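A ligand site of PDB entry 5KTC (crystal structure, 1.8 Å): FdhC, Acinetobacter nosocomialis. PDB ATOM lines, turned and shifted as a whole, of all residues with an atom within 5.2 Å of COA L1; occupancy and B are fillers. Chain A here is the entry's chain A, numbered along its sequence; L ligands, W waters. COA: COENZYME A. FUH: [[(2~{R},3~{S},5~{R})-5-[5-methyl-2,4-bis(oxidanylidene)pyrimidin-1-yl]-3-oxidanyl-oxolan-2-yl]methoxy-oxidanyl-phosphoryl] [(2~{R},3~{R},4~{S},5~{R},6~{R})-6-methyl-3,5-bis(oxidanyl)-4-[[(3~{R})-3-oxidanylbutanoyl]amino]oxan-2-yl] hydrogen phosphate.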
ATOM      1  N   LEU A  33     -27.522  22.122  33.238  1.00  0.00           N
ATOM      2  CA  LEU A  33     -27.330  22.798  31.970  1.00  0.00           C
ATOM      3  C   LEU A  33     -27.120  24.271  32.076  1.00  0.00           C
ATOM      4  O   LEU A  33     -26.559  24.856  31.157  1.00  0.00           O
ATOM      5  CB  LEU A  33     -28.567  22.545  31.083  1.00  0.00           C
ATOM      6  CG  LEU A  33     -28.790  21.054  30.768  1.00  0.00           C
ATOM      7  CD1 LEU A  33     -30.047  20.911  29.876  1.00  0.00           C
ATOM      8  CD2 LEU A  33     -27.599  20.360  30.082  1.00  0.00           C
ATOM      9  N   TYR A  36     -23.925  28.403  32.925  1.00  0.00           N
ATOM     10  CA  TYR A  36     -23.337  29.561  32.235  1.00  0.00           C
ATOM     11  C   TYR A  36     -24.344  30.328  31.335  1.00  0.00           C
ATOM     12  O   TYR A  36     -23.946  31.011  30.349  1.00  0.00           O
ATOM     13  CB  TYR A  36     -22.176  29.054  31.428  1.00  0.00           C
ATOM     14  CG  TYR A  36     -21.101  28.364  32.231  1.00  0.00           C
ATOM     15  CD1 TYR A  36     -20.277  29.085  33.099  1.00  0.00           C
ATOM     16  CD2 TYR A  36     -20.886  27.023  32.092  1.00  0.00           C
ATOM     17  CE1 TYR A  36     -19.288  28.444  33.823  1.00  0.00           C
ATOM     18  CE2 TYR A  36     -19.898  26.390  32.777  1.00  0.00           C
ATOM     19  CZ  TYR A  36     -19.102  27.093  33.662  1.00  0.00           C
ATOM     20  OH  TYR A  36     -18.086  26.403  34.344  1.00  0.00           O
ATOM     21  N   ILE A  37     -25.624  30.194  31.644  1.00  0.00           N
ATOM     22  CA  ILE A  37     -26.626  30.948  30.935  1.00  0.00           C
ATOM     23  C   ILE A  37     -27.368  31.815  31.915  1.00  0.00           C
ATOM     24  O   ILE A  37     -27.180  31.657  33.135  1.00  0.00           O
ATOM     25  CB  ILE A  37     -27.557  30.045  30.081  1.00  0.00           C
ATOM     26  CG1 ILE A  37     -28.545  29.328  30.971  1.00  0.00           C
ATOM     27  CG2 ILE A  37     -26.705  29.035  29.313  1.00  0.00           C
ATOM     28  CD1 ILE A  37     -29.579  28.506  30.251  1.00  0.00           C
ATOM     29  N   TRP A  97     -27.866  28.766  23.687  1.00  0.00           N
ATOM     30  CA  TRP A  97     -27.524  27.535  22.975  1.00  0.00           C
ATOM     31  C   TRP A  97     -27.443  26.465  24.036  1.00  0.00           C
ATOM     32  O   TRP A  97     -26.501  26.464  24.884  1.00  0.00           O
ATOM     33  CB  TRP A  97     -26.197  27.673  22.316  1.00  0.00           C
ATOM     34  CG  TRP A  97     -25.795  26.530  21.427  1.00  0.00           C
ATOM     35  CD1 TRP A  97     -26.603  25.744  20.658  1.00  0.00           C
ATOM     36  CD2 TRP A  97     -24.455  26.105  21.187  1.00  0.00           C
ATOM     37  NE1 TRP A  97     -25.811  24.845  19.947  1.00  0.00           N
ATOM     38  CE2 TRP A  97     -24.499  25.062  20.239  1.00  0.00           C
ATOM     39  CE3 TRP A  97     -23.206  26.507  21.696  1.00  0.00           C
ATOM     40  CZ2 TRP A  97     -23.380  24.393  19.806  1.00  0.00           C
ATOM     41  CZ3 TRP A  97     -22.051  25.846  21.254  1.00  0.00           C
ATOM     42  CH2 TRP A  97     -22.159  24.802  20.287  1.00  0.00           C
ATOM     43  N   ILE A  98     -28.416  25.560  24.013  1.00  0.00           N
ATOM     44  CA  ILE A  98     -28.568  24.563  25.056  1.00  0.00           C
ATOM     45  C   ILE A  98     -28.968  23.230  24.431  1.00  0.00           C
ATOM     46  O   ILE A  98     -29.848  23.183  23.572  1.00  0.00           O
ATOM     47  CB  ILE A  98     -29.625  24.912  26.112  1.00  0.00           C
ATOM     48  CG1 ILE A  98     -29.482  26.358  26.635  1.00  0.00           C
ATOM     49  CG2 ILE A  98     -29.440  23.975  27.283  1.00  0.00           C
ATOM     50  CD1 ILE A  98     -30.658  26.944  27.348  1.00  0.00           C
ATOM     51  N   LEU A  99     -28.282  22.178  24.846  1.00  0.00           N
ATOM     52  CA  LEU A  99     -28.655  20.806  24.428  1.00  0.00           C
ATOM     53  C   LEU A  99     -28.800  19.907  25.687  1.00  0.00           C
ATOM     54  O   LEU A  99     -27.927  19.948  26.545  1.00  0.00           O
ATOM     55  CB  LEU A  99     -27.589  20.246  23.508  1.00  0.00           C
ATOM     56  CG  LEU A  99     -27.544  20.828  22.089  1.00  0.00           C
ATOM     57  CD1 LEU A  99     -26.309  20.340  21.387  1.00  0.00           C
ATOM     58  CD2 LEU A  99     -28.780  20.491  21.256  1.00  0.00           C
ATOM     59  N   LYS A 103     -29.794  14.671  23.503  1.00  0.00           N
ATOM     60  CA  LYS A 103     -29.192  15.167  22.297  1.00  0.00           C
ATOM     61  C   LYS A 103     -28.511  14.012  21.541  1.00  0.00           C
ATOM     62  O   LYS A 103     -28.009  13.072  22.150  1.00  0.00           O
ATOM     63  CB  LYS A 103     -28.124  16.262  22.636  1.00  0.00           C
ATOM     64  CG  LYS A 103     -26.892  15.713  23.385  1.00  0.00           C
ATOM     65  CD  LYS A 103     -25.906  16.752  23.848  1.00  0.00           C
ATOM     66  CE  LYS A 103     -24.766  16.111  24.661  1.00  0.00           C
ATOM     67  NZ  LYS A 103     -23.936  17.135  25.370  1.00  0.00           N
ATOM     68  N   LYS A 105     -25.237  12.724  19.421  1.00  0.00           N
ATOM     69  CA  LYS A 105     -23.817  12.868  19.807  1.00  0.00           C
ATOM     70  C   LYS A 105     -23.195  14.178  19.274  1.00  0.00           C
ATOM     71  O   LYS A 105     -22.495  14.878  20.016  1.00  0.00           O
ATOM     72  CB  LYS A 105     -23.003  11.723  19.256  1.00  0.00           C
ATOM     73  CG  LYS A 105     -21.608  11.654  19.821  1.00  0.00           C
ATOM     74  CD  LYS A 105     -20.989  10.310  19.466  1.00  0.00           C
ATOM     75  CE  LYS A 105     -19.521  10.220  19.891  1.00  0.00           C
ATOM     76  NZ  LYS A 105     -19.317  10.331  21.365  1.00  0.00           N
ATOM     77  N   TYR A 106     -23.467  14.438  17.996  1.00  0.00           N
ATOM     78  CA  TYR A 106     -22.901  15.549  17.286  1.00  0.00           C
ATOM     79  C   TYR A 106     -23.899  16.695  17.094  1.00  0.00           C
ATOM     80  O   TYR A 106     -23.657  17.556  16.265  1.00  0.00           O
ATOM     81  CB  TYR A 106     -22.308  15.077  15.906  1.00  0.00           C
ATOM     82  CG  TYR A 106     -21.232  14.008  16.103  1.00  0.00           C
ATOM     83  CD1 TYR A 106     -20.091  14.288  16.843  1.00  0.00           C
ATOM     84  CD2 TYR A 106     -21.380  12.711  15.593  1.00  0.00           C
ATOM     85  CE1 TYR A 106     -19.125  13.313  17.084  1.00  0.00           C
ATOM     86  CE2 TYR A 106     -20.414  11.732  15.853  1.00  0.00           C
ATOM     87  CZ  TYR A 106     -19.302  12.032  16.568  1.00  0.00           C
ATOM     88  OH  TYR A 106     -18.336  11.078  16.845  1.00  0.00           O
ATOM     89  N   ALA A 108     -24.299  19.314  18.741  1.00  0.00           N
ATOM     90  CA  ALA A 108     -23.627  20.624  18.985  1.00  0.00           C
ATOM     91  C   ALA A 108     -23.014  21.128  17.678  1.00  0.00           C
ATOM     92  O   ALA A 108     -23.210  22.293  17.276  1.00  0.00           O
ATOM     93  CB  ALA A 108     -22.593  20.530  20.117  1.00  0.00           C
ATOM     94  N   VAL A 109     -22.314  20.249  16.984  1.00  0.00           N
ATOM     95  CA  VAL A 109     -21.716  20.607  15.685  1.00  0.00           C
ATOM     96  C   VAL A 109     -22.794  20.946  14.660  1.00  0.00           C
ATOM     97  O   VAL A 109     -22.697  21.955  13.929  1.00  0.00           O
ATOM     98  CB  VAL A 109     -20.795  19.484  15.126  1.00  0.00           C
ATOM     99  CG1 VAL A 109     -20.190  19.894  13.819  1.00  0.00           C
ATOM    100  CG2 VAL A 109     -19.725  19.116  16.114  1.00  0.00           C
ATOM    101  N   GLU A 131     -20.639  35.543  22.953  1.00  0.00           N
ATOM    102  CA  GLU A 131     -19.774  35.444  24.119  1.00  0.00           C
ATOM    103  C   GLU A 131     -19.987  34.130  24.867  1.00  0.00           C
ATOM    104  O   GLU A 131     -21.037  33.503  24.734  1.00  0.00           O
ATOM    105  CB  GLU A 131     -20.040  36.611  25.051  1.00  0.00           C
ATOM    106  CG  GLU A 131     -21.402  36.757  25.640  1.00  0.00           C
ATOM    107  CD  GLU A 131     -22.337  37.703  24.941  1.00  0.00           C
ATOM    108  OE1 GLU A 131     -23.554  37.492  25.006  1.00  0.00           O
ATOM    109  OE2 GLU A 131     -21.876  38.672  24.325  1.00  0.00           O
ATOM    110  N   VAL A 132     -18.986  33.740  25.668  1.00  0.00           N
ATOM    111  CA  VAL A 132     -18.987  32.497  26.406  1.00  0.00           C
ATOM    112  C   VAL A 132     -18.380  32.793  27.768  1.00  0.00           C
ATOM    113  O   VAL A 132     -17.345  33.473  27.853  1.00  0.00           O
ATOM    114  CB  VAL A 132     -18.090  31.482  25.717  1.00  0.00           C
ATOM    115  CG1 VAL A 132     -18.042  30.158  26.457  1.00  0.00           C
ATOM    116  CG2 VAL A 132     -18.528  31.277  24.258  1.00  0.00           C
ATOM    117  N   MET A 133     -19.028  32.371  28.838  1.00  0.00           N
ATOM    118  CA  MET A 133     -18.486  32.651  30.178  1.00  0.00           C
ATOM    119  C   MET A 133     -17.156  32.025  30.416  1.00  0.00           C
ATOM    120  O   MET A 133     -16.923  30.914  30.050  1.00  0.00           O
ATOM    121  CB  MET A 133     -19.450  32.233  31.288  1.00  0.00           C
ATOM    122  CG  MET A 133     -20.594  33.237  31.488  1.00  0.00           C
ATOM    123  SD  MET A 133     -21.525  32.936  33.012  1.00  0.00           S
ATOM    124  CE  MET A 133     -20.435  33.636  34.278  1.00  0.00           C
ATOM    125  N   ASN A 136     -16.430  28.087  31.131  1.00  0.00           N
ATOM    126  CA  ASN A 136     -17.165  27.163  30.227  1.00  0.00           C
ATOM    127  C   ASN A 136     -16.252  26.570  29.171  1.00  0.00           C
ATOM    128  O   ASN A 136     -16.405  26.726  27.928  1.00  0.00           O
ATOM    129  CB  ASN A 136     -18.355  27.909  29.602  1.00  0.00           C
ATOM    130  CG  ASN A 136     -19.502  26.988  29.170  1.00  0.00           C
ATOM    131  OD1 ASN A 136     -19.427  25.775  29.278  1.00  0.00           O
ATOM    132  ND2 ASN A 136     -20.556  27.594  28.675  1.00  0.00           N
ATOM    133  N   LYS A 138     -15.040  23.871  27.762  1.00  0.00           N
ATOM    134  CA  LYS A 138     -15.278  23.075  26.597  1.00  0.00           C
ATOM    135  C   LYS A 138     -15.966  23.894  25.443  1.00  0.00           C
ATOM    136  O   LYS A 138     -15.874  23.558  24.270  1.00  0.00           O
ATOM    137  CB  LYS A 138     -16.135  21.870  27.037  1.00  0.00           C
ATOM    138  CG  LYS A 138     -16.189  20.808  26.013  1.00  0.00           C
ATOM    139  CD  LYS A 138     -16.756  19.478  26.501  1.00  0.00           C
ATOM    140  CE  LYS A 138     -16.757  18.579  25.266  1.00  0.00           C
ATOM    141  NZ  LYS A 138     -17.346  17.236  25.484  1.00  0.00           N
ATOM    142  N   VAL A 139     -16.723  24.911  25.811  1.00  0.00           N
ATOM    143  CA  VAL A 139     -17.455  25.746  24.816  1.00  0.00           C
ATOM    144  C   VAL A 139     -16.473  26.718  24.147  1.00  0.00           C
ATOM    145  O   VAL A 139     -16.517  26.927  22.945  1.00  0.00           O
ATOM    146  CB  VAL A 139     -18.667  26.433  25.501  1.00  0.00           C
ATOM    147  CG1 VAL A 139     -19.434  27.358  24.527  1.00  0.00           C
ATOM    148  CG2 VAL A 139     -19.577  25.348  26.051  1.00  0.00           C
ATOM    149  N   PHE A 142     -14.704  24.455  21.704  1.00  0.00           N
ATOM    150  CA  PHE A 142     -15.551  24.222  20.567  1.00  0.00           C
ATOM    151  C   PHE A 142     -15.482  25.334  19.532  1.00  0.00           C
ATOM    152  O   PHE A 142     -15.319  25.067  18.372  1.00  0.00           O
ATOM    153  CB  PHE A 142     -17.039  24.101  21.028  1.00  0.00           C
ATOM    154  CG  PHE A 142     -18.007  23.861  19.902  1.00  0.00           C
ATOM    155  CD1 PHE A 142     -18.539  24.905  19.154  1.00  0.00           C
ATOM    156  CD2 PHE A 142     -18.404  22.553  19.591  1.00  0.00           C
ATOM    157  CE1 PHE A 142     -19.426  24.650  18.115  1.00  0.00           C
ATOM    158  CE2 PHE A 142     -19.284  22.303  18.563  1.00  0.00           C
ATOM    159  CZ  PHE A 142     -19.795  23.354  17.816  1.00  0.00           C
ATOM    160  N   LYS A 145     -12.048  25.774  17.904  1.00  0.00           N
ATOM    161  CA  LYS A 145     -11.882  24.720  16.928  1.00  0.00           C
ATOM    162  C   LYS A 145     -12.614  25.000  15.625  1.00  0.00           C
ATOM    163  O   LYS A 145     -12.088  24.790  14.541  1.00  0.00           O
ATOM    164  CB  LYS A 145     -12.327  23.367  17.479  1.00  0.00           C
ATOM    165  CG  LYS A 145     -12.026  22.145  16.564  1.00  0.00           C
ATOM    166  CD  LYS A 145     -12.195  20.833  17.363  1.00  0.00           C
ATOM    167  CE  LYS A 145     -12.062  19.552  16.532  1.00  0.00           C
ATOM    168  NZ  LYS A 145     -10.790  19.498  15.730  1.00  0.00           N
ATOM    169  N   MET A 146     -13.860  25.432  15.701  1.00  0.00           N
ATOM    170  CA  MET A 146     -14.619  25.699  14.457  1.00  0.00           C
ATOM    171  C   MET A 146     -14.131  26.969  13.723  1.00  0.00           C
ATOM    172  O   MET A 146     -14.478  27.192  12.583  1.00  0.00           O
ATOM    173  CB  MET A 146     -16.122  25.866  14.798  1.00  0.00           C
ATOM    174  CG  MET A 146     -17.053  25.895  13.598  1.00  0.00           C
ATOM    175  SD  MET A 146     -18.780  25.748  14.131  1.00  0.00           S
ATOM    176  CE  MET A 146     -18.888  23.999  14.514  1.00  0.00           C
ATOM    177  N   TYR A 174     -16.922  20.484   6.859  1.00  0.00           N
ATOM    178  CA  TYR A 174     -17.950  19.953   7.761  1.00  0.00           C
ATOM    179  C   TYR A 174     -19.200  19.422   7.018  1.00  0.00           C
ATOM    180  O   TYR A 174     -20.260  19.198   7.651  1.00  0.00           O
ATOM    181  CB  TYR A 174     -18.384  21.036   8.760  1.00  0.00           C
ATOM    182  CG  TYR A 174     -17.376  21.379   9.816  1.00  0.00           C
ATOM    183  CD1 TYR A 174     -16.298  22.229   9.558  1.00  0.00           C
ATOM    184  CD2 TYR A 174     -17.489  20.816  11.056  1.00  0.00           C
ATOM    185  CE1 TYR A 174     -15.362  22.540  10.567  1.00  0.00           C
ATOM    186  CE2 TYR A 174     -16.574  21.106  12.061  1.00  0.00           C
ATOM    187  CZ  TYR A 174     -15.518  21.975  11.818  1.00  0.00           C
ATOM    188  OH  TYR A 174     -14.687  22.214  12.865  1.00  0.00           O
ATOM    189  N   ARG A 176     -19.958  16.492   6.079  1.00  0.00           N
ATOM    190  CA  ARG A 176     -20.423  15.217   6.637  1.00  0.00           C
ATOM    191  C   ARG A 176     -21.472  15.395   7.778  1.00  0.00           C
ATOM    192  O   ARG A 176     -22.195  14.446   8.129  1.00  0.00           O
ATOM    193  CB  ARG A 176     -19.273  14.333   7.139  1.00  0.00           C
ATOM    194  CG  ARG A 176     -18.520  14.846   8.331  1.00  0.00           C
ATOM    195  CD  ARG A 176     -17.356  13.969   8.568  1.00  0.00           C
ATOM    196  NE  ARG A 176     -16.509  14.458   9.598  1.00  0.00           N
ATOM    197  CZ  ARG A 176     -16.556  14.124  10.878  1.00  0.00           C
ATOM    198  NH1 ARG A 176     -17.465  13.261  11.344  1.00  0.00           N
ATOM    199  NH2 ARG A 176     -15.679  14.683  11.687  1.00  0.00           N
ATOM    200  N   PHE A 177     -21.434  16.541   8.452  1.00  0.00           N
ATOM    201  CA  PHE A 177     -22.378  16.811   9.530  1.00  0.00           C
ATOM    202  C   PHE A 177     -23.730  17.335   9.034  1.00  0.00           C
ATOM    203  O   PHE A 177     -24.722  17.300   9.758  1.00  0.00           O
ATOM    204  CB  PHE A 177     -21.760  17.815  10.506  1.00  0.00           C
ATOM    205  CG  PHE A 177     -20.620  17.279  11.301  1.00  0.00           C
ATOM    206  CD1 PHE A 177     -20.851  16.537  12.444  1.00  0.00           C
ATOM    207  CD2 PHE A 177     -19.332  17.593  10.929  1.00  0.00           C
ATOM    208  CE1 PHE A 177     -19.824  16.052  13.212  1.00  0.00           C
ATOM    209  CE2 PHE A 177     -18.283  17.131  11.692  1.00  0.00           C
ATOM    210  CZ  PHE A 177     -18.529  16.360  12.838  1.00  0.00           C
HETATM  211  N1A COA L   1     -15.247  18.811  14.695  1.00  0.00           N
HETATM  212  C2A COA L   1     -15.566  17.515  14.947  1.00  0.00           C
HETATM  213  N3A COA L   1     -16.140  17.132  16.096  1.00  0.00           N
HETATM  214  C4A COA L   1     -16.487  18.058  16.977  1.00  0.00           C
HETATM  215  C5A COA L   1     -16.202  19.489  16.744  1.00  0.00           C
HETATM  216  C6A COA L   1     -15.532  19.830  15.512  1.00  0.00           C
HETATM  217  N6A COA L   1     -15.229  21.094  15.212  1.00  0.00           N
HETATM  218  N7A COA L   1     -16.662  20.163  17.787  1.00  0.00           N
HETATM  219  C8A COA L   1     -17.179  19.251  18.642  1.00  0.00           C
HETATM  220  N9A COA L   1     -17.064  17.995  18.155  1.00  0.00           N
HETATM  221  C1B COA L   1     -17.535  16.742  18.780  1.00  0.00           C
HETATM  222  C2B COA L   1     -17.176  16.746  20.268  1.00  0.00           C
HETATM  223  O2B COA L   1     -15.851  16.254  20.525  1.00  0.00           O
HETATM  224  C3B COA L   1     -18.272  15.923  20.861  1.00  0.00           C
HETATM  225  O3B COA L   1     -17.976  14.551  20.589  1.00  0.00           O
HETATM  226  P3B COA L   1     -17.495  13.578  21.775  1.00  0.00           P
HETATM  227  O7A COA L   1     -18.815  12.887  22.146  1.00  0.00           O
HETATM  228  O8A COA L   1     -16.580  12.790  20.880  1.00  0.00           O
HETATM  229  O9A COA L   1     -16.883  14.436  22.852  1.00  0.00           O
HETATM  230  C4B COA L   1     -19.479  16.315  20.035  1.00  0.00           C
HETATM  231  O4B COA L   1     -18.972  16.694  18.744  1.00  0.00           O
HETATM  232  C5B COA L   1     -20.348  17.363  20.699  1.00  0.00           C
HETATM  233  O5B COA L   1     -19.592  18.520  20.979  1.00  0.00           O
HETATM  234  P1A COA L   1     -19.454  19.036  22.463  1.00  0.00           P
HETATM  235  O1A COA L   1     -18.401  20.122  22.483  1.00  0.00           O
HETATM  236  O2A COA L   1     -19.486  17.956  23.515  1.00  0.00           O
HETATM  237  O3A COA L   1     -20.787  19.901  22.750  1.00  0.00           O
HETATM  238  P2A COA L   1     -22.024  19.660  23.670  1.00  0.00           P
HETATM  239  O4A COA L   1     -22.833  18.443  23.307  1.00  0.00           O
HETATM  240  O5A COA L   1     -21.657  19.776  25.142  1.00  0.00           O
HETATM  241  O6A COA L   1     -22.954  20.899  23.313  1.00  0.00           O
HETATM  242  CBP COA L   1     -23.594  22.965  24.433  1.00  0.00           C
HETATM  243  CCP COA L   1     -22.506  22.205  23.663  1.00  0.00           C
HETATM  244  CDP COA L   1     -23.017  24.304  24.819  1.00  0.00           C
HETATM  245  CEP COA L   1     -24.833  23.166  23.556  1.00  0.00           C
HETATM  246  CAP COA L   1     -23.986  22.150  25.686  1.00  0.00           C
HETATM  247  OAP COA L   1     -22.728  21.744  26.313  1.00  0.00           O
HETATM  248  C9P COA L   1     -24.887  22.856  26.624  1.00  0.00           C
HETATM  249  O9P COA L   1     -26.126  22.950  26.522  1.00  0.00           O
HETATM  250  N8P COA L   1     -24.237  23.450  27.652  1.00  0.00           N
HETATM  251  C7P COA L   1     -24.945  24.182  28.621  1.00  0.00           C
HETATM  252  C6P COA L   1     -25.530  25.501  28.170  1.00  0.00           C
HETATM  253  C5P COA L   1     -24.420  26.434  27.766  1.00  0.00           C
HETATM  254  O5P COA L   1     -23.463  26.606  28.549  1.00  0.00           O
HETATM  255  N4P COA L   1     -24.510  26.982  26.578  1.00  0.00           N
HETATM  256  C3P COA L   1     -23.434  27.805  26.017  1.00  0.00           C
HETATM  257  C2P COA L   1     -23.388  29.219  26.627  1.00  0.00           C
HETATM  258  S1P COA L   1     -21.852  30.056  26.068  1.00  0.00           S
HETATM  259  O1  FUH L   2     -25.129  30.804  24.154  1.00  0.00           O
HETATM  260  C1  FUH L   2     -24.259  31.661  24.077  1.00  0.00           C
HETATM  261  C2  FUH L   2     -23.263  31.723  22.969  1.00  0.00           C
HETATM  262  C3  FUH L   2     -23.062  30.382  22.307  1.00  0.00           C
HETATM  263  O2  FUH L   2     -21.999  29.637  22.935  1.00  0.00           O
HETATM  264  C4  FUH L   2     -22.661  30.565  20.863  1.00  0.00           C
HETATM  265  N1  FUH L   2     -24.151  32.680  25.028  1.00  0.00           N
HETATM  266  C5  FUH L   2     -25.247  32.933  25.962  1.00  0.00           C
HETATM  267  C6  FUH L   2     -24.725  33.141  27.399  1.00  0.00           C
HETATM  268  O3  FUH L   2     -23.817  34.157  27.356  1.00  0.00           O
HETATM  269  C7  FUH L   2     -25.790  33.604  28.369  1.00  0.00           C
HETATM  270  C8  FUH L   2     -25.238  34.089  29.733  1.00  0.00           C
HETATM  271  O4  FUH L   2     -26.529  34.694  27.820  1.00  0.00           O
HETATM  272  C9  FUH L   2     -26.010  34.174  25.519  1.00  0.00           C
HETATM  273  O5  FUH L   2     -26.697  33.968  24.281  1.00  0.00           O
HETATM  274  C10 FUH L   2     -27.062  34.488  26.506  1.00  0.00           C
HETATM  275  O6  FUH L   2     -27.972  33.394  26.511  1.00  0.00           O
HETATM  276  P1  FUH L   2     -29.374  33.486  27.212  1.00  0.00           P
HETATM  277  O7  FUH L   2     -29.301  33.255  28.676  1.00  0.00           O
HETATM  278  O8  FUH L   2     -30.190  32.387  26.517  1.00  0.00           O
HETATM  279  O9  FUH L   2     -30.165  34.790  26.753  1.00  0.00           O
HETATM  280  P2  FUH L   2     -30.127  36.304  27.273  1.00  0.00           P
HETATM  281  O10 FUH L   2     -29.937  37.172  26.088  1.00  0.00           O
HETATM  282  O11 FUH L   2     -29.001  36.383  28.298  1.00  0.00           O
HETATM  283  O12 FUH L   2     -31.574  36.391  27.872  1.00  0.00           O
HETATM  284  C11 FUH L   2     -32.221  37.659  28.016  1.00  0.00           C
HETATM  285  C12 FUH L   2     -33.188  37.572  29.168  1.00  0.00           C
HETATM  286  C13 FUH L   2     -32.602  36.899  30.429  1.00  0.00           C
HETATM  287  O13 FUH L   2     -33.128  37.480  31.636  1.00  0.00           O
HETATM  288  C14 FUH L   2     -33.121  35.475  30.391  1.00  0.00           C
HETATM  289  C15 FUH L   2     -34.446  35.658  29.697  1.00  0.00           C
HETATM  290  O14 FUH L   2     -34.317  36.785  28.786  1.00  0.00           O
HETATM  291  N2  FUH L   2     -34.900  34.566  28.809  1.00  0.00           N
HETATM  292  C16 FUH L   2     -34.213  34.255  27.678  1.00  0.00           C
HETATM  293  C17 FUH L   2     -34.693  33.258  26.823  1.00  0.00           C
HETATM  294  C18 FUH L   2     -33.989  32.884  25.544  1.00  0.00           C
HETATM  295  C19 FUH L   2     -35.892  32.582  27.215  1.00  0.00           C
HETATM  296  O15 FUH L   2     -36.397  31.687  26.424  1.00  0.00           O
HETATM  297  N3  FUH L   2     -36.544  32.916  28.340  1.00  0.00           N
HETATM  298  C20 FUH L   2     -36.067  33.908  29.092  1.00  0.00           C
HETATM  299  O16 FUH L   2     -36.705  34.214  30.211  1.00  0.00           O
HETATM  300  O   HOH W   1     -24.284  26.279  31.263  1.00  0.00           O
HETATM  301  O   HOH W   2     -21.543  14.217  22.469  1.00  0.00           O
HETATM  302  O   HOH W   3     -18.678  22.430  23.854  1.00  0.00           O
HETATM  303  O   HOH W   4     -16.350  22.988  17.177  1.00  0.00           O
HETATM  304  O   HOH W   5     -21.717  31.642  28.835  1.00  0.00           O
HETATM  305  O   HOH W   6     -21.458  23.949  28.943  1.00  0.00           O
HETATM  306  O   HOH W   7     -23.795  17.432  20.852  1.00  0.00           O
HETATM  307  O   HOH W   8     -14.345  20.982  20.155  1.00  0.00           O
HETATM  308  O   HOH W   9     -23.685  20.334  28.626  1.00  0.00           O
HETATM  309  O   HOH W  10     -19.564  21.120  25.880  1.00  0.00           O
HETATM  310  O   HOH W  11     -13.843  18.318  19.161  1.00  0.00           O
HETATM  311  O   HOH W  12     -21.176  16.005  24.599  1.00  0.00           O
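An oxygen (O7A) of COA L1 lies within salt-bridge range of the side-chain amino group (NZ) of Lys 105, at 2.7 Å.
The backbone NH (N) of Leu 99 is in hydrogen-bond range of an oxygen (O9P) of COA L1 (2.8 Å).
An oxygen (O2A) of COA L1 lies within salt-bridge range of the side-chain amino group (NZ) of Lys 138 (3.0 Å).
N4P of COA L1 lies within hydrogen-bond range of O of Trp 97 (2.7 Å).
A sulfur (S1P) of COA L1 sits close to the backbone carbonyl oxygen (O) of Glu 131 (3.8 Å).
The side-chain hydroxyl (OH) of Tyr 174 is in hydrogen-bond range of a nitrogen (N6A) of COA L1 (2.7 Å).
The backbone NH (N) of Trp 97 is in hydrogen-bond range of an oxygen (O1) of FUH L2 (3.4 Å).
O of Glu 131 sits at hydrogen-bond distance from N1 of FUH L2.
NZ of Lys 103 is in salt-bridge range of O4A of COA L1 (2.7 Å).
ND2 of Asn 136 lies within hydrogen-bond range of O5P of COA L1 (3.1 Å).
A sulfur (S1P) of COA L1 sits close to an oxygen (O2) of FUH L2 (3.2 Å).
Leu 33 touches COA L1 (O to C7P, 3.1 Å).
Tyr 36 touches COA L1 (CB to O5P, 3.99 Å).
Ile 37 touches COA L1.
Ile 98 touches COA L1.
CD1 of Tyr 106 touches O4B of COA L1, at 3.3 Å.
Ala 108 touches COA L1.
Val 109 touches COA L1 (CG2 to C4A, 3.5 Å).
Val 132 touches COA L1.
Val 139 touches COA L1.
Phe 142 touches COA L1 (CD2 to N7A, 3.5 Å).
Lys 145 touches COA L1 (CE to C6A, 3.6 Å).
CZ of Phe 177 touches C2A of COA L1 (3.8 Å).
Hydrophobic or aromatic side chains within 4 Å of COA L1: Tyr 36, Ile 37, Trp 97, Ile 98, Leu 99, Tyr 106, Ala 108, Val 109, Val 132, Val 139, Phe 142, Tyr 174 and Phe 177.
Within 4 Å of COA L1: Leu 33, Tyr 36, Ile 37, Trp 97, Ile 98, Leu 99, Lys 103, Lys 105, Tyr 106, Ala 108, Val 109, Glu 131, Val 132, Asn 136, Lys 138, Val 139, Phe 142, Lys 145, Tyr 174 and Phe 177.
Water W3 bridges an oxygen (O1A) of COA L1 (2.7 Å) and the backbone carbonyl oxygen (O) of Lys 138 (3.1 Å).
Water W7 lies within hydrogen-bond range of an oxygen (O4A) of COA L1 (2.8 Å), the backbone NH of Ala 108 (2.9 Å) and the backbone carbonyl oxygen of Lys 105 (3.0 Å).
Water W1 lies within hydrogen-bond range of the backbone carbonyl oxygen (O) of Leu 33 (2.7 Å), the backbone NH (N) of Tyr 36 (2.7 Å) and an oxygen (O5P) of COA L1 (2.9 Å).
Water W2 lies within hydrogen-bond range of the backbone carbonyl oxygen (O) of Lys 105 and an oxygen (O7A) of COA L1.
Water W6 lies within hydrogen-bond range of the side-chain amide oxygen (OD1) of Asn 136 (2.8 Å) and a nitrogen (N8P) of COA L1 (3.1 Å).
Water W5 lies within hydrogen-bond range of O of Tyr 36 (2.8 Å), N of Met 133 (2.8 Å) and S1P of COA L1 (3.2 Å).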
